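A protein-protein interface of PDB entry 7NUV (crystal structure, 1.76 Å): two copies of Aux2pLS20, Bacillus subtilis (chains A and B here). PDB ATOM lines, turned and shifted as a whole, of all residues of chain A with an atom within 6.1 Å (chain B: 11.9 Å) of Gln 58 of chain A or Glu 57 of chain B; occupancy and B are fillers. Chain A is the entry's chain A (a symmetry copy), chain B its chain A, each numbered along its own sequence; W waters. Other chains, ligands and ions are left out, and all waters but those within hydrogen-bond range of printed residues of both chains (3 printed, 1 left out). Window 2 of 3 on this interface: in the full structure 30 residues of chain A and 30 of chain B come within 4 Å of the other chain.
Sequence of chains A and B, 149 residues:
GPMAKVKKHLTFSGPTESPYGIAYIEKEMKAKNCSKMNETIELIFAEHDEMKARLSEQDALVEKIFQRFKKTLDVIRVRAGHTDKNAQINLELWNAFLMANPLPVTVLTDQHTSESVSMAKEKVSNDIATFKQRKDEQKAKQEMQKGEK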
ATOM      1  N   SER A  56     -16.726  20.183  11.415  1.00  0.00           N
ATOM      2  CA  SER A  56     -15.891  21.324  11.764  1.00  0.00           C
ATOM      3  C   SER A  56     -16.402  22.578  11.060  1.00  0.00           C
ATOM      4  O   SER A  56     -17.169  22.514  10.091  1.00  0.00           O
ATOM      5  CB  SER A  56     -14.435  21.080  11.376  1.00  0.00           C
ATOM      6  OG  SER A  56     -14.268  21.102   9.965  1.00  0.00           O
ATOM      7  N   GLU A  57     -15.967  23.739  11.560  1.00  0.00           N
ATOM      8  CA  GLU A  57     -16.365  24.990  10.922  1.00  0.00           C
ATOM      9  C   GLU A  57     -15.930  25.016   9.465  1.00  0.00           C
ATOM     10  O   GLU A  57     -16.725  25.323   8.571  1.00  0.00           O
ATOM     11  CB  GLU A  57     -15.782  26.188  11.673  1.00  0.00           C
ATOM     12  CG  GLU A  57     -16.595  27.471  11.508  1.00  0.00           C
ATOM     13  CD  GLU A  57     -16.865  27.829  10.041  1.00  0.00           C
ATOM     14  OE1 GLU A  57     -15.952  28.380   9.380  1.00  0.00           O
ATOM     15  OE2 GLU A  57     -17.983  27.542   9.541  1.00  0.00           O
ATOM     16  N   GLN A  58     -14.667  24.689   9.208  1.00  0.00           N
ATOM     17  CA  GLN A  58     -14.161  24.742   7.846  1.00  0.00           C
ATOM     18  C   GLN A  58     -14.871  23.746   6.941  1.00  0.00           C
ATOM     19  O   GLN A  58     -15.199  24.066   5.788  1.00  0.00           O
ATOM     20  CB  GLN A  58     -12.659  24.501   7.862  1.00  0.00           C
ATOM     21  CG  GLN A  58     -12.021  24.530   6.505  1.00  0.00           C
ATOM     22  CD  GLN A  58     -10.527  24.370   6.601  1.00  0.00           C
ATOM     23  OE1 GLN A  58      -9.999  23.260   6.520  1.00  0.00           O
ATOM     24  NE2 GLN A  58      -9.826  25.489   6.762  1.00  0.00           N
ATOM     25  N   ASP A  59     -15.112  22.527   7.435  1.00  0.00           N
ATOM     26  CA  ASP A  59     -15.803  21.535   6.620  1.00  0.00           C
ATOM     27  C   ASP A  59     -17.252  21.930   6.388  1.00  0.00           C
ATOM     28  O   ASP A  59     -17.811  21.622   5.332  1.00  0.00           O
ATOM     29  CB  ASP A  59     -15.721  20.152   7.272  1.00  0.00           C
ATOM     30  CG  ASP A  59     -14.361  19.482   7.069  1.00  0.00           C
ATOM     31  OD1 ASP A  59     -13.411  20.153   6.602  1.00  0.00           O
ATOM     32  OD2 ASP A  59     -14.236  18.285   7.404  1.00  0.00           O
ATOM     33  N   ALA A  60     -17.869  22.622   7.347  1.00  0.00           N
ATOM     34  CA  ALA A  60     -19.218  23.130   7.119  1.00  0.00           C
ATOM     35  C   ALA A  60     -19.227  24.158   5.992  1.00  0.00           C
ATOM     36  O   ALA A  60     -20.158  24.187   5.174  1.00  0.00           O
ATOM     37  CB  ALA A  60     -19.788  23.721   8.412  1.00  0.00           C
ATOM     38  N   LEU A  61     -18.194  25.002   5.926  1.00  0.00           N
ATOM     39  CA  LEU A  61     -18.073  25.960   4.829  1.00  0.00           C
ATOM     40  C   LEU A  61     -17.860  25.242   3.507  1.00  0.00           C
ATOM     41  O   LEU A  61     -18.504  25.559   2.500  1.00  0.00           O
ATOM     42  CB  LEU A  61     -16.911  26.923   5.085  1.00  0.00           C
ATOM     43  CG  LEU A  61     -16.506  27.810   3.902  1.00  0.00           C
ATOM     44  CD1 LEU A  61     -17.677  28.698   3.495  1.00  0.00           C
ATOM     45  CD2 LEU A  61     -15.284  28.649   4.232  1.00  0.00           C
ATOM     46  N   VAL A  62     -16.951  24.267   3.496  1.00  0.00           N
ATOM     47  CA  VAL A  62     -16.662  23.533   2.265  1.00  0.00           C
ATOM     48  C   VAL A  62     -17.932  22.870   1.760  1.00  0.00           C
ATOM     49  O   VAL A  62     -18.230  22.871   0.559  1.00  0.00           O
ATOM     50  CB  VAL A  62     -15.557  22.492   2.522  1.00  0.00           C
ATOM     51  CG1 VAL A  62     -15.597  21.370   1.459  1.00  0.00           C
ATOM     52  CG2 VAL A  62     -14.172  23.146   2.658  1.00  0.00           C
ATOM     53  N   GLU A  63     -18.714  22.310   2.676  1.00  0.00           N
ATOM     54  CA  GLU A  63     -19.896  21.580   2.258  1.00  0.00           C
ATOM     55  C   GLU A  63     -20.951  22.550   1.730  1.00  0.00           C
ATOM     56  O   GLU A  63     -21.657  22.241   0.761  1.00  0.00           O
ATOM     57  CB  GLU A  63     -20.435  20.788   3.446  1.00  0.00           C
ATOM     58  CG  GLU A  63     -21.718  20.017   3.213  1.00  0.00           C
ATOM     59  CD  GLU A  63     -21.537  18.953   2.120  1.00  0.00           C
ATOM     60  OE1 GLU A  63     -22.540  18.526   1.504  1.00  0.00           O
ATOM     61  OE2 GLU A  63     -20.375  18.521   1.900  1.00  0.00           O
ATOM     62  N   LEU B  55       0.973  23.201   4.030  1.00  0.00           N
ATOM     63  CA  LEU B  55       0.287  24.246   3.283  1.00  0.00           C
ATOM     64  C   LEU B  55      -0.117  25.381   4.224  1.00  0.00           C
ATOM     65  O   LEU B  55      -0.295  25.156   5.423  1.00  0.00           O
ATOM     66  CB  LEU B  55      -0.952  23.675   2.596  1.00  0.00           C
ATOM     67  CG  LEU B  55      -0.765  22.664   1.457  1.00  0.00           C
ATOM     68  CD1 LEU B  55      -2.068  21.878   1.270  1.00  0.00           C
ATOM     69  CD2 LEU B  55      -0.324  23.333   0.154  1.00  0.00           C
ATOM     70  N   SER B  56      -0.268  26.593   3.691  1.00  0.00           N
ATOM     71  CA  SER B  56      -0.870  27.666   4.469  1.00  0.00           C
ATOM     72  C   SER B  56      -2.311  27.309   4.824  1.00  0.00           C
ATOM     73  O   SER B  56      -2.927  26.418   4.226  1.00  0.00           O
ATOM     74  CB  SER B  56      -0.849  28.984   3.697  1.00  0.00           C
ATOM     75  OG  SER B  56      -1.761  28.956   2.608  1.00  0.00           O
ATOM     76  N   GLU B  57      -2.854  28.018   5.818  1.00  0.00           N
ATOM     77  CA  GLU B  57      -4.243  27.778   6.197  1.00  0.00           C
ATOM     78  C   GLU B  57      -5.172  28.006   5.014  1.00  0.00           C
ATOM     79  O   GLU B  57      -6.026  27.168   4.707  1.00  0.00           O
ATOM     80  CB  GLU B  57      -4.645  28.674   7.370  1.00  0.00           C
ATOM     81  CG  GLU B  57      -5.780  28.101   8.218  1.00  0.00           C
ATOM     82  CD  GLU B  57      -7.009  27.704   7.391  1.00  0.00           C
ATOM     83  OE1 GLU B  57      -7.803  28.604   7.026  1.00  0.00           O
ATOM     84  OE2 GLU B  57      -7.174  26.494   7.089  1.00  0.00           O
ATOM     85  N   GLN B  58      -5.014  29.138   4.334  1.00  0.00           N
ATOM     86  CA  GLN B  58      -5.899  29.452   3.224  1.00  0.00           C
ATOM     87  C   GLN B  58      -5.758  28.450   2.087  1.00  0.00           C
ATOM     88  O   GLN B  58      -6.760  28.034   1.488  1.00  0.00           O
ATOM     89  CB  GLN B  58      -5.619  30.871   2.749  1.00  0.00           C
ATOM     90  CG  GLN B  58      -6.474  31.310   1.598  1.00  0.00           C
ATOM     91  CD  GLN B  58      -6.205  32.746   1.235  1.00  0.00           C
ATOM     92  OE1 GLN B  58      -5.377  33.040   0.372  1.00  0.00           O
ATOM     93  NE2 GLN B  58      -6.918  33.660   1.887  1.00  0.00           N
ATOM     94  N   ASP B  59      -4.521  28.056   1.764  1.00  0.00           N
ATOM     95  CA  ASP B  59      -4.324  27.085   0.695  1.00  0.00           C
ATOM     96  C   ASP B  59      -4.858  25.718   1.089  1.00  0.00           C
ATOM     97  O   ASP B  59      -5.332  24.971   0.228  1.00  0.00           O
ATOM     98  CB  ASP B  59      -2.843  26.995   0.317  1.00  0.00           C
ATOM     99  CG  ASP B  59      -2.383  28.164  -0.556  1.00  0.00           C
ATOM    100  OD1 ASP B  59      -3.142  29.149  -0.709  1.00  0.00           O
ATOM    101  OD2 ASP B  59      -1.245  28.107  -1.068  1.00  0.00           O
ATOM    102  N   ALA B  60      -4.808  25.380   2.379  1.00  0.00           N
ATOM    103  CA  ALA B  60      -5.420  24.132   2.823  1.00  0.00           C
ATOM    104  C   ALA B  60      -6.930  24.161   2.607  1.00  0.00           C
ATOM    105  O   ALA B  60      -7.530  23.149   2.217  1.00  0.00           O
ATOM    106  CB  ALA B  60      -5.076  23.866   4.292  1.00  0.00           C
ATOM    107  N   LEU B  61      -7.560  25.315   2.844  1.00  0.00           N
ATOM    108  CA  LEU B  61      -8.989  25.462   2.578  1.00  0.00           C
ATOM    109  C   LEU B  61      -9.275  25.353   1.090  1.00  0.00           C
ATOM    110  O   LEU B  61     -10.200  24.647   0.670  1.00  0.00           O
ATOM    111  CB  LEU B  61      -9.495  26.808   3.103  1.00  0.00           C
ATOM    112  CG  LEU B  61     -10.910  27.206   2.664  1.00  0.00           C
ATOM    113  CD1 LEU B  61     -11.917  26.178   3.167  1.00  0.00           C
ATOM    114  CD2 LEU B  61     -11.271  28.597   3.153  1.00  0.00           C
ATOM    115  N   VAL B  62      -8.483  26.052   0.276  1.00  0.00           N
ATOM    116  CA  VAL B  62      -8.695  26.027  -1.170  1.00  0.00           C
ATOM    117  C   VAL B  62      -8.583  24.597  -1.673  1.00  0.00           C
ATOM    118  O   VAL B  62      -9.371  24.143  -2.512  1.00  0.00           O
ATOM    119  CB  VAL B  62      -7.670  26.940  -1.866  1.00  0.00           C
ATOM    120  CG1 VAL B  62      -7.494  26.545  -3.350  1.00  0.00           C
ATOM    121  CG2 VAL B  62      -8.004  28.430  -1.673  1.00  0.00           C
ATOM    122  N   GLU B  63      -7.612  23.857  -1.150  1.00  0.00           N
ATOM    123  CA  GLU B  63      -7.389  22.513  -1.649  1.00  0.00           C
ATOM    124  C   GLU B  63      -8.530  21.597  -1.212  1.00  0.00           C
ATOM    125  O   GLU B  63      -8.955  20.719  -1.975  1.00  0.00           O
ATOM    126  CB  GLU B  63      -6.052  22.004  -1.117  1.00  0.00           C
ATOM    127  CG  GLU B  63      -5.685  20.579  -1.479  1.00  0.00           C
ATOM    128  CD  GLU B  63      -5.560  20.405  -3.000  1.00  0.00           C
ATOM    129  OE1 GLU B  63      -5.686  19.265  -3.501  1.00  0.00           O
ATOM    130  OE2 GLU B  63      -5.304  21.424  -3.694  1.00  0.00           O
ATOM    131  N   LYS B  64      -9.060  21.816   0.000  1.00  0.00           N
ATOM    132  CA  LYS B  64     -10.159  20.996   0.509  1.00  0.00           C
ATOM    133  C   LYS B  64     -11.436  21.215  -0.301  1.00  0.00           C
ATOM    134  O   LYS B  64     -12.138  20.257  -0.649  1.00  0.00           O
ATOM    135  CB  LYS B  64     -10.385  21.312   1.985  1.00  0.00           C
ATOM    136  CG  LYS B  64     -11.317  20.365   2.691  1.00  0.00           C
ATOM    137  CD  LYS B  64     -10.567  19.661   3.815  1.00  0.00           C
ATOM    138  CE  LYS B  64     -10.317  20.619   4.969  1.00  0.00           C
ATOM    139  NZ  LYS B  64     -10.439  19.954   6.303  1.00  0.00           N
ATOM    140  N   ILE B  65     -11.741  22.475  -0.615  1.00  0.00           N
ATOM    141  CA  ILE B  65     -12.838  22.793  -1.525  1.00  0.00           C
ATOM    142  C   ILE B  65     -12.647  22.090  -2.866  1.00  0.00           C
ATOM    143  O   ILE B  65     -13.532  21.372  -3.348  1.00  0.00           O
ATOM    144  CB  ILE B  65     -12.924  24.314  -1.703  1.00  0.00           C
ATOM    145  CG1 ILE B  65     -13.402  24.951  -0.395  1.00  0.00           C
ATOM    146  CG2 ILE B  65     -13.799  24.661  -2.925  1.00  0.00           C
ATOM    147  CD1 ILE B  65     -13.070  26.422  -0.290  1.00  0.00           C
ATOM    148  N   PHE B  66     -11.484  22.291  -3.487  1.00  0.00           N
ATOM    149  CA  PHE B  66     -11.261  21.813  -4.851  1.00  0.00           C
ATOM    150  C   PHE B  66     -11.302  20.294  -4.939  1.00  0.00           C
ATOM    151  O   PHE B  66     -11.789  19.739  -5.933  1.00  0.00           O
ATOM    152  CB  PHE B  66      -9.932  22.375  -5.367  1.00  0.00           C
ATOM    153  CG  PHE B  66      -9.614  22.034  -6.813  1.00  0.00           C
ATOM    154  CD1 PHE B  66     -10.565  22.194  -7.812  1.00  0.00           C
ATOM    155  CD2 PHE B  66      -8.329  21.666  -7.174  1.00  0.00           C
ATOM    156  CE1 PHE B  66     -10.250  21.896  -9.149  1.00  0.00           C
ATOM    157  CE2 PHE B  66      -8.004  21.388  -8.514  1.00  0.00           C
ATOM    158  CZ  PHE B  66      -8.976  21.514  -9.490  1.00  0.00           C
ATOM    159  N   GLN B  67     -10.820  19.598  -3.911  1.00  0.00           N
ATOM    160  CA  GLN B  67     -10.791  18.142  -3.992  1.00  0.00           C
ATOM    161  C   GLN B  67     -12.186  17.539  -3.986  1.00  0.00           C
ATOM    162  O   GLN B  67     -12.339  16.365  -4.335  1.00  0.00           O
ATOM    163  CB  GLN B  67      -9.972  17.552  -2.844  1.00  0.00           C
ATOM    164  CG  GLN B  67      -8.484  17.533  -3.113  1.00  0.00           C
ATOM    165  CD  GLN B  67      -7.679  17.200  -1.869  1.00  0.00           C
ATOM    166  OE1 GLN B  67      -8.139  17.423  -0.743  1.00  0.00           O
ATOM    167  NE2 GLN B  67      -6.463  16.695  -2.060  1.00  0.00           N
ATOM    168  N   ARG B  68     -13.203  18.313  -3.618  1.00  0.00           N
ATOM    169  CA  ARG B  68     -14.555  17.782  -3.676  1.00  0.00           C
ATOM    170  C   ARG B  68     -15.021  17.569  -5.117  1.00  0.00           C
ATOM    171  O   ARG B  68     -15.922  16.753  -5.351  1.00  0.00           O
ATOM    172  CB  ARG B  68     -15.508  18.713  -2.933  1.00  0.00           C
ATOM    173  CG  ARG B  68     -15.349  18.626  -1.395  1.00  0.00           C
ATOM    174  CD  ARG B  68     -15.495  17.185  -0.904  1.00  0.00           C
ATOM    175  NE  ARG B  68     -16.867  16.688  -0.872  1.00  0.00           N
ATOM    176  CZ  ARG B  68     -17.769  16.999   0.052  1.00  0.00           C
ATOM    177  NH1 ARG B  68     -17.489  17.839   1.040  1.00  0.00           N
ATOM    178  NH2 ARG B  68     -18.978  16.441  -0.009  1.00  0.00           N
HETATM  179  O   HOH W   1     -11.414  20.655   9.470  1.00  0.00           O
HETATM  180  O   HOH W   2     -11.853  17.390   7.106  1.00  0.00           O
HETATM  181  O   HOH W   3     -22.276  15.904   0.071  1.00  0.00           O
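NZ of Lys 64 of chain B sits close to OE1 of Gln 58 of chain A, at 3.3 Å. The side-chain amino group of Lys 64 of chain B is in salt-bridge range of the side-chain carboxylate of Asp 59 of chain A (3.0 Å). The side-chain amide nitrogen (NE2) of Gln 58 of chain A lies within hydrogen-bond range of the side-chain carboxylate (OE2) of Glu 57 of chain B, 2.9 Å away. NH1 of Arg 68 of chain B lies within salt-bridge range of OE2 of Glu 63 of chain A (3.1 Å).
N of Asp 59 of chain A lies within hydrogen-bond range of OG of Ser 56 of chain A (3.0 Å).
Among the printed residues, merely in contact across the chains: Val 62 of chain A with Ile 65 of chain B (3.6 Å), Gln 58 of chain A with Leu 61 of chain B (3.7 Å), Val 62 of chain A with Leu 61 of chain B (3.8 Å), Val 62 of chain A with Arg 68 of chain B (3.97 Å) and Val 62 of chain A with Lys 64 of chain B (3.99 Å).
Glu 57 of chain B touches just one residue of chain A: Gln 58. No residue of chain B comes within 4 Å of Ser 56 of chain A. No residue of chain B comes within 4 Å of Glu 57 of chain A. Asp 59 of chain A touches just one residue of chain B: Lys 64. No residue of chain B comes within 4 Å of Ala 60 of chain A. No residue of chain B comes within 4 Å of Leu 61 of chain A. Of the printed residues of chain B, Val 62 of chain A touches Leu 61, Lys 64, Ile 65 and Arg 68. Of the printed residues of chain A, Arg 68 of chain B touches Val 62 and Glu 63. Of the printed residues of chain B, Glu 63 of chain A touches Arg 68. The nearest residue of chain B that does not touch Gln 58 of chain A is Ala 60 of chain B (5.0 Å). The nearest printed residue of chain A that does not touch Glu 57 of chain B is Leu 61 of chain A (8.0 Å).
Of the 14 printed residues of chain B, 5 touch a printed residue of chain A. Printed residues of chain B that touch a printed residue of chain A: Glu 57, Leu 61, Lys 64, Ile 65 and Arg 68. Hydrophobic or aromatic side chains of chain B within 4 Å of the printed part of chain A: Leu 61 and Ile 65. Among the printed residues, 9 pairs touch across the chains.
Gln 58 of chain A touches Glu 57 of chain B, but with the chains exchanged Glu 57 of chain A does not touch Gln 58 of chain B (11.8 Å). Gln 58 of chain A touches Leu 61 of chain B, but with the chains exchanged Leu 61 of chain A does not touch Gln 58 of chain B (9.0 Å). Val 62 of chain A touches Leu 61 of chain B, but with the chains exchanged Leu 61 of chain A does not touch Val 62 of chain B (8.3 Å). Positions printed for both chains: 56, 57, 58, 59, 60, 61, 62 and 63.
Water W2 lies within hydrogen-bond range of OD2 of Asp 59 of chain A (2.6 Å) and NZ of Lys 64 of chain B (3.0 Å). Water W1 lies within hydrogen-bond range of OG of Ser 56 of chain A (2.9 Å) and NZ of Lys 64 of chain B (3.4 Å). Water W3 lies within hydrogen-bond range of OE1 of Glu 63 of chain A (3.0 Å) and NH2 of Arg 68 of chain B (3.3 Å).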
